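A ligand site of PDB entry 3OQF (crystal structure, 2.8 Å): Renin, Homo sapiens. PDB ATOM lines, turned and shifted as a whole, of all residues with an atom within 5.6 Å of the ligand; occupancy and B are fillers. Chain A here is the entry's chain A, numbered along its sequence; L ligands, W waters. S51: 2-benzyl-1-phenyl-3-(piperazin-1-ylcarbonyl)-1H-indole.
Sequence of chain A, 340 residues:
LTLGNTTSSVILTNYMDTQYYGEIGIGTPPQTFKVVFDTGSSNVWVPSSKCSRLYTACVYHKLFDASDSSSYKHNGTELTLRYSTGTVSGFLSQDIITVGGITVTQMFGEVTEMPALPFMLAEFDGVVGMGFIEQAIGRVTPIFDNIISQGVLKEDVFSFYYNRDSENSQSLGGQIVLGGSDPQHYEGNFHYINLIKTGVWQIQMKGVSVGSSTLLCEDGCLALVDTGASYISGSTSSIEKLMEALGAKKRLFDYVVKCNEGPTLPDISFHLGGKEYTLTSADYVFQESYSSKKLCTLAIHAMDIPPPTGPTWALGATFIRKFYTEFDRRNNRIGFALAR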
ATOM      1  N   THR A  18      -4.131 -25.865   0.577  1.00  0.00           N
ATOM      2  CA  THR A  18      -5.000 -25.742  -0.588  1.00  0.00           C
ATOM      3  C   THR A  18      -4.366 -24.949  -1.730  1.00  0.00           C
ATOM      4  O   THR A  18      -4.696 -25.185  -2.892  1.00  0.00           O
ATOM      5  CB  THR A  18      -6.360 -25.170  -0.195  1.00  0.00           C
ATOM      6  OG1 THR A  18      -6.196 -23.856   0.355  1.00  0.00           O
ATOM      7  CG2 THR A  18      -7.096 -26.036   0.778  1.00  0.00           C
ATOM      8  N   GLN A  19      -3.521 -23.973  -1.400  1.00  0.00           N
ATOM      9  CA  GLN A  19      -2.892 -23.118  -2.397  1.00  0.00           C
ATOM     10  C   GLN A  19      -1.402 -23.070  -2.181  1.00  0.00           C
ATOM     11  O   GLN A  19      -0.934 -22.750  -1.096  1.00  0.00           O
ATOM     12  CB  GLN A  19      -3.488 -21.700  -2.375  1.00  0.00           C
ATOM     13  CG  GLN A  19      -5.008 -21.653  -2.532  1.00  0.00           C
ATOM     14  CD  GLN A  19      -5.585 -20.276  -2.467  1.00  0.00           C
ATOM     15  OE1 GLN A  19      -4.966 -19.311  -2.900  1.00  0.00           O
ATOM     16  NE2 GLN A  19      -6.797 -20.160  -1.969  1.00  0.00           N
ATOM     17  N   VAL A  36       0.603 -19.429  -9.094  1.00  0.00           N
ATOM     18  CA  VAL A  36       0.517 -20.880  -9.002  1.00  0.00           C
ATOM     19  C   VAL A  36       1.246 -21.420 -10.226  1.00  0.00           C
ATOM     20  O   VAL A  36       1.065 -20.903 -11.333  1.00  0.00           O
ATOM     21  CB  VAL A  36      -0.947 -21.389  -8.975  1.00  0.00           C
ATOM     22  CG1 VAL A  36      -1.012 -22.913  -9.074  1.00  0.00           C
ATOM     23  CG2 VAL A  36      -1.639 -20.939  -7.716  1.00  0.00           C
ATOM     24  N   ASP A  38       1.213 -24.347 -12.525  1.00  0.00           N
ATOM     25  CA  ASP A  38       0.135 -25.227 -12.936  1.00  0.00           C
ATOM     26  C   ASP A  38       0.421 -26.124 -14.145  1.00  0.00           C
ATOM     27  O   ASP A  38       0.424 -25.639 -15.277  1.00  0.00           O
ATOM     28  CB  ASP A  38      -1.100 -24.334 -13.182  1.00  0.00           C
ATOM     29  CG  ASP A  38      -2.364 -25.064 -13.564  1.00  0.00           C
ATOM     30  OD1 ASP A  38      -2.456 -26.266 -13.299  1.00  0.00           O
ATOM     31  OD2 ASP A  38      -3.259 -24.424 -14.136  1.00  0.00           O
ATOM     32  N   GLY A  40      -1.613 -28.260 -15.196  1.00  0.00           N
ATOM     33  CA  GLY A  40      -2.917 -28.415 -15.819  1.00  0.00           C
ATOM     34  C   GLY A  40      -3.258 -27.355 -16.854  1.00  0.00           C
ATOM     35  O   GLY A  40      -4.341 -27.402 -17.442  1.00  0.00           O
ATOM     36  N   SER A  41      -2.372 -26.366 -17.058  1.00  0.00           N
ATOM     37  CA  SER A  41      -2.575 -25.302 -18.049  1.00  0.00           C
ATOM     38  C   SER A  41      -1.224 -24.884 -18.641  1.00  0.00           C
ATOM     39  O   SER A  41      -0.181 -25.281 -18.115  1.00  0.00           O
ATOM     40  CB  SER A  41      -3.388 -24.128 -17.510  1.00  0.00           C
ATOM     41  OG  SER A  41      -2.690 -23.411 -16.500  1.00  0.00           O
ATOM     42  N   TRP A  45      -0.480 -15.772 -16.949  1.00  0.00           N
ATOM     43  CA  TRP A  45      -1.292 -14.559 -16.823  1.00  0.00           C
ATOM     44  C   TRP A  45      -1.207 -13.963 -15.442  1.00  0.00           C
ATOM     45  O   TRP A  45      -0.997 -14.670 -14.458  1.00  0.00           O
ATOM     46  CB  TRP A  45      -2.754 -14.738 -17.275  1.00  0.00           C
ATOM     47  CG  TRP A  45      -3.597 -15.627 -16.411  1.00  0.00           C
ATOM     48  CD1 TRP A  45      -3.923 -16.925 -16.651  1.00  0.00           C
ATOM     49  CD2 TRP A  45      -4.285 -15.268 -15.194  1.00  0.00           C
ATOM     50  NE1 TRP A  45      -4.745 -17.401 -15.659  1.00  0.00           N
ATOM     51  CE2 TRP A  45      -4.976 -16.408 -14.744  1.00  0.00           C
ATOM     52  CE3 TRP A  45      -4.358 -14.086 -14.427  1.00  0.00           C
ATOM     53  CZ2 TRP A  45      -5.748 -16.408 -13.569  1.00  0.00           C
ATOM     54  CZ3 TRP A  45      -5.111 -14.092 -13.262  1.00  0.00           C
ATOM     55  CH2 TRP A  45      -5.794 -15.243 -12.839  1.00  0.00           C
ATOM     56  N   TYR A  83     -11.173 -22.283 -17.238  1.00  0.00           N
ATOM     57  CA  TYR A  83     -10.774 -23.336 -16.310  1.00  0.00           C
ATOM     58  C   TYR A  83     -12.011 -23.996 -15.751  1.00  0.00           C
ATOM     59  O   TYR A  83     -13.114 -23.512 -15.963  1.00  0.00           O
ATOM     60  CB  TYR A  83      -9.899 -22.803 -15.170  1.00  0.00           C
ATOM     61  CG  TYR A  83      -8.681 -22.056 -15.674  1.00  0.00           C
ATOM     62  CD1 TYR A  83      -7.498 -22.734 -15.964  1.00  0.00           C
ATOM     63  CD2 TYR A  83      -8.740 -20.691 -15.912  1.00  0.00           C
ATOM     64  CE1 TYR A  83      -6.370 -22.059 -16.441  1.00  0.00           C
ATOM     65  CE2 TYR A  83      -7.629 -20.004 -16.407  1.00  0.00           C
ATOM     66  CZ  TYR A  83      -6.444 -20.698 -16.667  1.00  0.00           C
ATOM     67  OH  TYR A  83      -5.349 -20.015 -17.150  1.00  0.00           O
ATOM     68  N   SER A  84     -11.817 -25.116 -15.052  1.00  0.00           N
ATOM     69  CA  SER A  84     -12.886 -25.876 -14.429  1.00  0.00           C
ATOM     70  C   SER A  84     -13.601 -25.043 -13.371  1.00  0.00           C
ATOM     71  O   SER A  84     -14.805 -25.195 -13.180  1.00  0.00           O
ATOM     72  CB  SER A  84     -12.326 -27.154 -13.829  1.00  0.00           C
ATOM     73  OG  SER A  84     -12.042 -28.109 -14.846  1.00  0.00           O
ATOM     74  N   THR A  85     -12.862 -24.165 -12.698  1.00  0.00           N
ATOM     75  CA  THR A  85     -13.402 -23.339 -11.618  1.00  0.00           C
ATOM     76  C   THR A  85     -13.897 -21.983 -12.063  1.00  0.00           C
ATOM     77  O   THR A  85     -14.646 -21.328 -11.334  1.00  0.00           O
ATOM     78  CB  THR A  85     -12.348 -23.139 -10.558  1.00  0.00           C
ATOM     79  OG1 THR A  85     -11.169 -22.584 -11.175  1.00  0.00           O
ATOM     80  CG2 THR A  85     -12.044 -24.403  -9.800  1.00  0.00           C
ATOM     81  N   GLY A  86     -13.423 -21.520 -13.218  1.00  0.00           N
ATOM     82  CA  GLY A  86     -13.817 -20.218 -13.699  1.00  0.00           C
ATOM     83  C   GLY A  86     -13.053 -19.753 -14.915  1.00  0.00           C
ATOM     84  O   GLY A  86     -12.182 -20.460 -15.426  1.00  0.00           O
ATOM     85  N   PRO A 118     -14.041 -17.555  -8.746  1.00  0.00           N
ATOM     86  CA  PRO A 118     -13.316 -17.937  -7.518  1.00  0.00           C
ATOM     87  C   PRO A 118     -12.158 -17.034  -7.082  1.00  0.00           C
ATOM     88  O   PRO A 118     -11.505 -17.336  -6.081  1.00  0.00           O
ATOM     89  CB  PRO A 118     -12.756 -19.315  -7.917  1.00  0.00           C
ATOM     90  CG  PRO A 118     -12.372 -19.111  -9.366  1.00  0.00           C
ATOM     91  CD  PRO A 118     -13.377 -18.135  -9.934  1.00  0.00           C
ATOM     92  N   PHE A 119     -11.863 -15.990  -7.847  1.00  0.00           N
ATOM     93  CA  PHE A 119     -10.655 -15.190  -7.660  1.00  0.00           C
ATOM     94  C   PHE A 119     -10.520 -14.367  -6.405  1.00  0.00           C
ATOM     95  O   PHE A 119      -9.394 -14.074  -6.010  1.00  0.00           O
ATOM     96  CB  PHE A 119     -10.244 -14.467  -8.940  1.00  0.00           C
ATOM     97  CG  PHE A 119      -9.954 -15.445 -10.055  1.00  0.00           C
ATOM     98  CD1 PHE A 119      -8.792 -16.207 -10.054  1.00  0.00           C
ATOM     99  CD2 PHE A 119     -10.858 -15.628 -11.085  1.00  0.00           C
ATOM    100  CE1 PHE A 119      -8.541 -17.141 -11.057  1.00  0.00           C
ATOM    101  CE2 PHE A 119     -10.603 -16.551 -12.095  1.00  0.00           C
ATOM    102  CZ  PHE A 119      -9.448 -17.301 -12.068  1.00  0.00           C
ATOM    103  N   LEU A 121     -11.029 -15.644  -3.708  1.00  0.00           N
ATOM    104  CA  LEU A 121     -10.578 -16.704  -2.813  1.00  0.00           C
ATOM    105  C   LEU A 121      -9.099 -17.089  -3.030  1.00  0.00           C
ATOM    106  O   LEU A 121      -8.543 -17.856  -2.236  1.00  0.00           O
ATOM    107  CB  LEU A 121     -11.448 -17.953  -2.951  1.00  0.00           C
ATOM    108  CG  LEU A 121     -12.933 -17.845  -2.619  1.00  0.00           C
ATOM    109  CD1 LEU A 121     -13.570 -19.203  -2.631  1.00  0.00           C
ATOM    110  CD2 LEU A 121     -13.154 -17.225  -1.255  1.00  0.00           C
ATOM    111  N   ALA A 122      -8.487 -16.575  -4.109  1.00  0.00           N
ATOM    112  CA  ALA A 122      -7.103 -16.830  -4.452  1.00  0.00           C
ATOM    113  C   ALA A 122      -6.178 -15.927  -3.637  1.00  0.00           C
ATOM    114  O   ALA A 122      -6.353 -14.707  -3.609  1.00  0.00           O
ATOM    115  CB  ALA A 122      -6.889 -16.610  -5.945  1.00  0.00           C
ATOM    116  N   PHE A 124      -3.065 -16.057  -4.371  1.00  0.00           N
ATOM    117  CA  PHE A 124      -2.161 -15.780  -5.455  1.00  0.00           C
ATOM    118  C   PHE A 124      -2.799 -14.753  -6.399  1.00  0.00           C
ATOM    119  O   PHE A 124      -4.025 -14.587  -6.411  1.00  0.00           O
ATOM    120  CB  PHE A 124      -1.808 -17.080  -6.202  1.00  0.00           C
ATOM    121  CG  PHE A 124      -3.007 -17.821  -6.752  1.00  0.00           C
ATOM    122  CD1 PHE A 124      -3.631 -18.819  -6.009  1.00  0.00           C
ATOM    123  CD2 PHE A 124      -3.494 -17.539  -8.027  1.00  0.00           C
ATOM    124  CE1 PHE A 124      -4.735 -19.519  -6.525  1.00  0.00           C
ATOM    125  CE2 PHE A 124      -4.602 -18.231  -8.544  1.00  0.00           C
ATOM    126  CZ  PHE A 124      -5.204 -19.230  -7.790  1.00  0.00           C
ATOM    127  N   VAL A 127      -1.074 -17.068 -12.596  1.00  0.00           N
ATOM    128  CA  VAL A 127      -0.695 -18.445 -12.895  1.00  0.00           C
ATOM    129  C   VAL A 127       0.436 -18.523 -13.891  1.00  0.00           C
ATOM    130  O   VAL A 127       0.471 -17.744 -14.855  1.00  0.00           O
ATOM    131  CB  VAL A 127      -1.936 -19.206 -13.471  1.00  0.00           C
ATOM    132  CG1 VAL A 127      -1.664 -20.695 -13.677  1.00  0.00           C
ATOM    133  CG2 VAL A 127      -3.202 -18.986 -12.632  1.00  0.00           C
ATOM    134  N   ASP A 226      -2.009 -32.745 -11.890  1.00  0.00           N
ATOM    135  CA  ASP A 226      -2.291 -31.328 -11.866  1.00  0.00           C
ATOM    136  C   ASP A 226      -1.826 -30.579 -10.631  1.00  0.00           C
ATOM    137  O   ASP A 226      -2.489 -30.601  -9.587  1.00  0.00           O
ATOM    138  CB  ASP A 226      -3.801 -31.140 -12.113  1.00  0.00           C
ATOM    139  CG  ASP A 226      -4.233 -29.726 -12.394  1.00  0.00           C
ATOM    140  OD1 ASP A 226      -3.360 -28.836 -12.434  1.00  0.00           O
ATOM    141  OD2 ASP A 226      -5.433 -29.503 -12.600  1.00  0.00           O
ATOM    142  N   GLY A 228      -1.803 -27.405 -10.180  1.00  0.00           N
ATOM    143  CA  GLY A 228      -2.675 -26.260  -9.921  1.00  0.00           C
ATOM    144  C   GLY A 228      -3.976 -26.630  -9.268  1.00  0.00           C
ATOM    145  O   GLY A 228      -4.776 -25.735  -8.983  1.00  0.00           O
ATOM    146  N   ALA A 229      -4.237 -27.920  -9.030  1.00  0.00           N
ATOM    147  CA  ALA A 229      -5.455 -28.400  -8.390  1.00  0.00           C
ATOM    148  C   ALA A 229      -5.201 -28.684  -6.902  1.00  0.00           C
ATOM    149  O   ALA A 229      -4.178 -29.286  -6.549  1.00  0.00           O
ATOM    150  CB  ALA A 229      -5.948 -29.664  -9.091  1.00  0.00           C
ATOM    151  N   SER A 230      -6.126 -28.234  -6.019  1.00  0.00           N
ATOM    152  CA  SER A 230      -5.980 -28.424  -4.571  1.00  0.00           C
ATOM    153  C   SER A 230      -6.198 -29.852  -4.128  1.00  0.00           C
ATOM    154  O   SER A 230      -5.509 -30.349  -3.227  1.00  0.00           O
ATOM    155  CB  SER A 230      -6.974 -27.544  -3.813  1.00  0.00           C
ATOM    156  OG  SER A 230      -6.813 -26.171  -4.117  1.00  0.00           O
ATOM    157  N   TYR A 231      -7.189 -30.515  -4.751  1.00  0.00           N
ATOM    158  CA  TYR A 231      -7.645 -31.837  -4.377  1.00  0.00           C
ATOM    159  C   TYR A 231      -7.393 -32.883  -5.414  1.00  0.00           C
ATOM    160  O   TYR A 231      -6.917 -32.596  -6.525  1.00  0.00           O
ATOM    161  CB  TYR A 231      -9.172 -31.761  -4.157  1.00  0.00           C
ATOM    162  CG  TYR A 231      -9.603 -30.834  -3.039  1.00  0.00           C
ATOM    163  CD1 TYR A 231     -10.640 -29.943  -3.217  1.00  0.00           C
ATOM    164  CD2 TYR A 231      -8.872 -30.748  -1.864  1.00  0.00           C
ATOM    165  CE1 TYR A 231     -11.040 -29.084  -2.196  1.00  0.00           C
ATOM    166  CE2 TYR A 231      -9.256 -29.914  -0.831  1.00  0.00           C
ATOM    167  CZ  TYR A 231     -10.385 -29.128  -0.979  1.00  0.00           C
ATOM    168  OH  TYR A 231     -10.765 -28.283   0.046  1.00  0.00           O
ATOM    169  N   HIS A 301     -12.969 -34.156  -4.395  1.00  0.00           N
ATOM    170  CA  HIS A 301     -14.296 -33.724  -4.840  1.00  0.00           C
ATOM    171  C   HIS A 301     -14.587 -34.084  -6.288  1.00  0.00           C
ATOM    172  O   HIS A 301     -13.733 -34.609  -6.990  1.00  0.00           O
ATOM    173  CB  HIS A 301     -14.522 -32.219  -4.571  1.00  0.00           C
ATOM    174  CG  HIS A 301     -13.597 -31.304  -5.323  1.00  0.00           C
ATOM    175  ND1 HIS A 301     -13.652 -29.932  -5.145  1.00  0.00           N
ATOM    176  CD2 HIS A 301     -12.619 -31.587  -6.233  1.00  0.00           C
ATOM    177  CE1 HIS A 301     -12.724 -29.420  -5.942  1.00  0.00           C
ATOM    178  NE2 HIS A 301     -12.070 -30.382  -6.611  1.00  0.00           N
ATOM    179  N   MET A 303     -15.235 -33.158 -10.157  1.00  0.00           N
ATOM    180  CA  MET A 303     -14.885 -32.171 -11.168  1.00  0.00           C
ATOM    181  C   MET A 303     -15.018 -32.805 -12.538  1.00  0.00           C
ATOM    182  O   MET A 303     -14.264 -33.716 -12.886  1.00  0.00           O
ATOM    183  CB  MET A 303     -13.487 -31.568 -10.969  1.00  0.00           C
ATOM    184  CG  MET A 303     -13.347 -30.229 -11.604  1.00  0.00           C
ATOM    185  SD  MET A 303     -13.754 -29.024 -10.333  1.00  0.00           S
ATOM    186  CE  MET A 303     -12.266 -28.047 -10.309  1.00  0.00           C
HETATM  187  C1  S51 L   1      -8.934 -20.573  -4.999  1.00  0.00           C
HETATM  188  C2  S51 L   1      -7.939 -21.545  -4.900  1.00  0.00           C
HETATM  189  C3  S51 L   1      -7.802 -22.500  -5.906  1.00  0.00           C
HETATM  190  C4  S51 L   1      -8.658 -22.581  -7.023  1.00  0.00           C
HETATM  191  C5  S51 L   1      -9.652 -21.590  -7.065  1.00  0.00           C
HETATM  192  C6  S51 L   1      -9.802 -20.591  -6.094  1.00  0.00           C
HETATM  193  N12 S51 L   1      -8.492 -23.550  -7.979  1.00  0.00           N
HETATM  194  C13 S51 L   1      -8.857 -24.833  -7.723  1.00  0.00           C
HETATM  195  C14 S51 L   1      -8.899 -25.461  -8.978  1.00  0.00           C
HETATM  196  C15 S51 L   1      -8.540 -24.504  -9.920  1.00  0.00           C
HETATM  197  C16 S51 L   1      -8.487 -23.242  -9.297  1.00  0.00           C
HETATM  198  C17 S51 L   1      -9.033 -25.606  -6.573  1.00  0.00           C
HETATM  199  C18 S51 L   1      -9.294 -26.978  -6.674  1.00  0.00           C
HETATM  200  C19 S51 L   1      -9.364 -27.593  -7.928  1.00  0.00           C
HETATM  201  C20 S51 L   1      -9.171 -26.838  -9.095  1.00  0.00           C
HETATM  202  C26 S51 L   1      -6.929 -22.002 -10.772  1.00  0.00           C
HETATM  203  C29 S51 L   1      -7.013 -21.711 -12.125  1.00  0.00           C
HETATM  204  C30 S51 L   1      -5.871 -21.863 -12.919  1.00  0.00           C
HETATM  205  C31 S51 L   1      -4.675 -22.315 -12.349  1.00  0.00           C
HETATM  206  C32 S51 L   1      -4.596 -22.618 -10.989  1.00  0.00           C
HETATM  207  C33 S51 L   1      -5.724 -22.461 -10.193  1.00  0.00           C
HETATM  208  C39 S51 L   1      -8.674 -24.821 -11.403  1.00  0.00           C
HETATM  209  N40 S51 L   1      -7.879 -25.696 -12.064  1.00  0.00           N
HETATM  210  O41 S51 L   1      -9.552 -24.212 -12.013  1.00  0.00           O
HETATM  211  C42 S51 L   1      -6.818 -26.483 -11.445  1.00  0.00           C
HETATM  212  C43 S51 L   1      -5.531 -26.191 -12.223  1.00  0.00           C
HETATM  213  N44 S51 L   1      -5.679 -26.375 -13.648  1.00  0.00           N
HETATM  214  C45 S51 L   1      -6.808 -25.723 -14.281  1.00  0.00           C
HETATM  215  C46 S51 L   1      -8.103 -25.975 -13.500  1.00  0.00           C
HETATM  216  C60 S51 L   1      -8.160 -21.889  -9.939  1.00  0.00           C
HETATM  217  O   HOH W   1      -9.118 -26.823 -16.620  1.00  0.00           O
HETATM  218  O   HOH W   2      -8.976 -30.840  -7.853  1.00  0.00           O
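N of Thr 85 sits close to O41 of the ligand (3.4 Å).
OG1 of Thr 85 lies within hydrogen-bond range of O41 of the ligand, 2.4 Å away.
The side-chain carboxylate (OD2) of Asp 38 lies within salt-bridge range of a nitrogen (N44) of the ligand (3.1 Å).
OD2 of Asp 226 is in salt-bridge range of N44 of the ligand.
N of Gly 228 lies within hydrogen-bond range of OD1 of Asp 38, at 3.4 Å.
N of Gly 40 is in hydrogen-bond range of OD1 of Asp 38, 2.9 Å away.
The side-chain carboxylate (OD2) of Asp 38 is in hydrogen-bond range of the side-chain hydroxyl (OG) of Ser 41 (2.6 Å).
N of Gly 40 sits at hydrogen-bond distance from OD1 of Asp 226, at 3.3 Å.
The side-chain hydroxyl (OG) of Ser 230 lies within hydrogen-bond range of the backbone carbonyl oxygen (O) of Thr 18 (2.6 Å).
The backbone carbonyl oxygen of Leu 121 is in hydrogen-bond range of the side-chain amide nitrogen of Gln 19.
OH of Tyr 83 lies within hydrogen-bond range of NE1 of Trp 45 (3.1 Å).
The backbone carbonyl oxygen (O) of Val 127 lies within hydrogen-bond range of the backbone NH (N) of Trp 45, at 3.0 Å.
Residues that only touch the ligand: Gly 228 (3.3 Å), Ser 230 (3.4 Å), Gln 19 (3.4 Å), Tyr 83 (3.5 Å), Met 303 (3.5 Å), Val 127 (3.7 Å), Pro 118 (3.7 Å), Ala 229 (3.8 Å), Leu 121 (3.9 Å) and Ser 84 (3.9 Å).
Hydrophobic or aromatic side chains within 4 Å of the ligand: Tyr 83, Pro 118, Val 127 and Met 303.
The nearest printed residue that does not touch the ligand is Phe 124 (4.1 Å).
Water W2 bridges the backbone carbonyl oxygen (O) of Tyr 231 (3.0 Å) and a ring nitrogen (NE2) of His 301 (3.4 Å).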
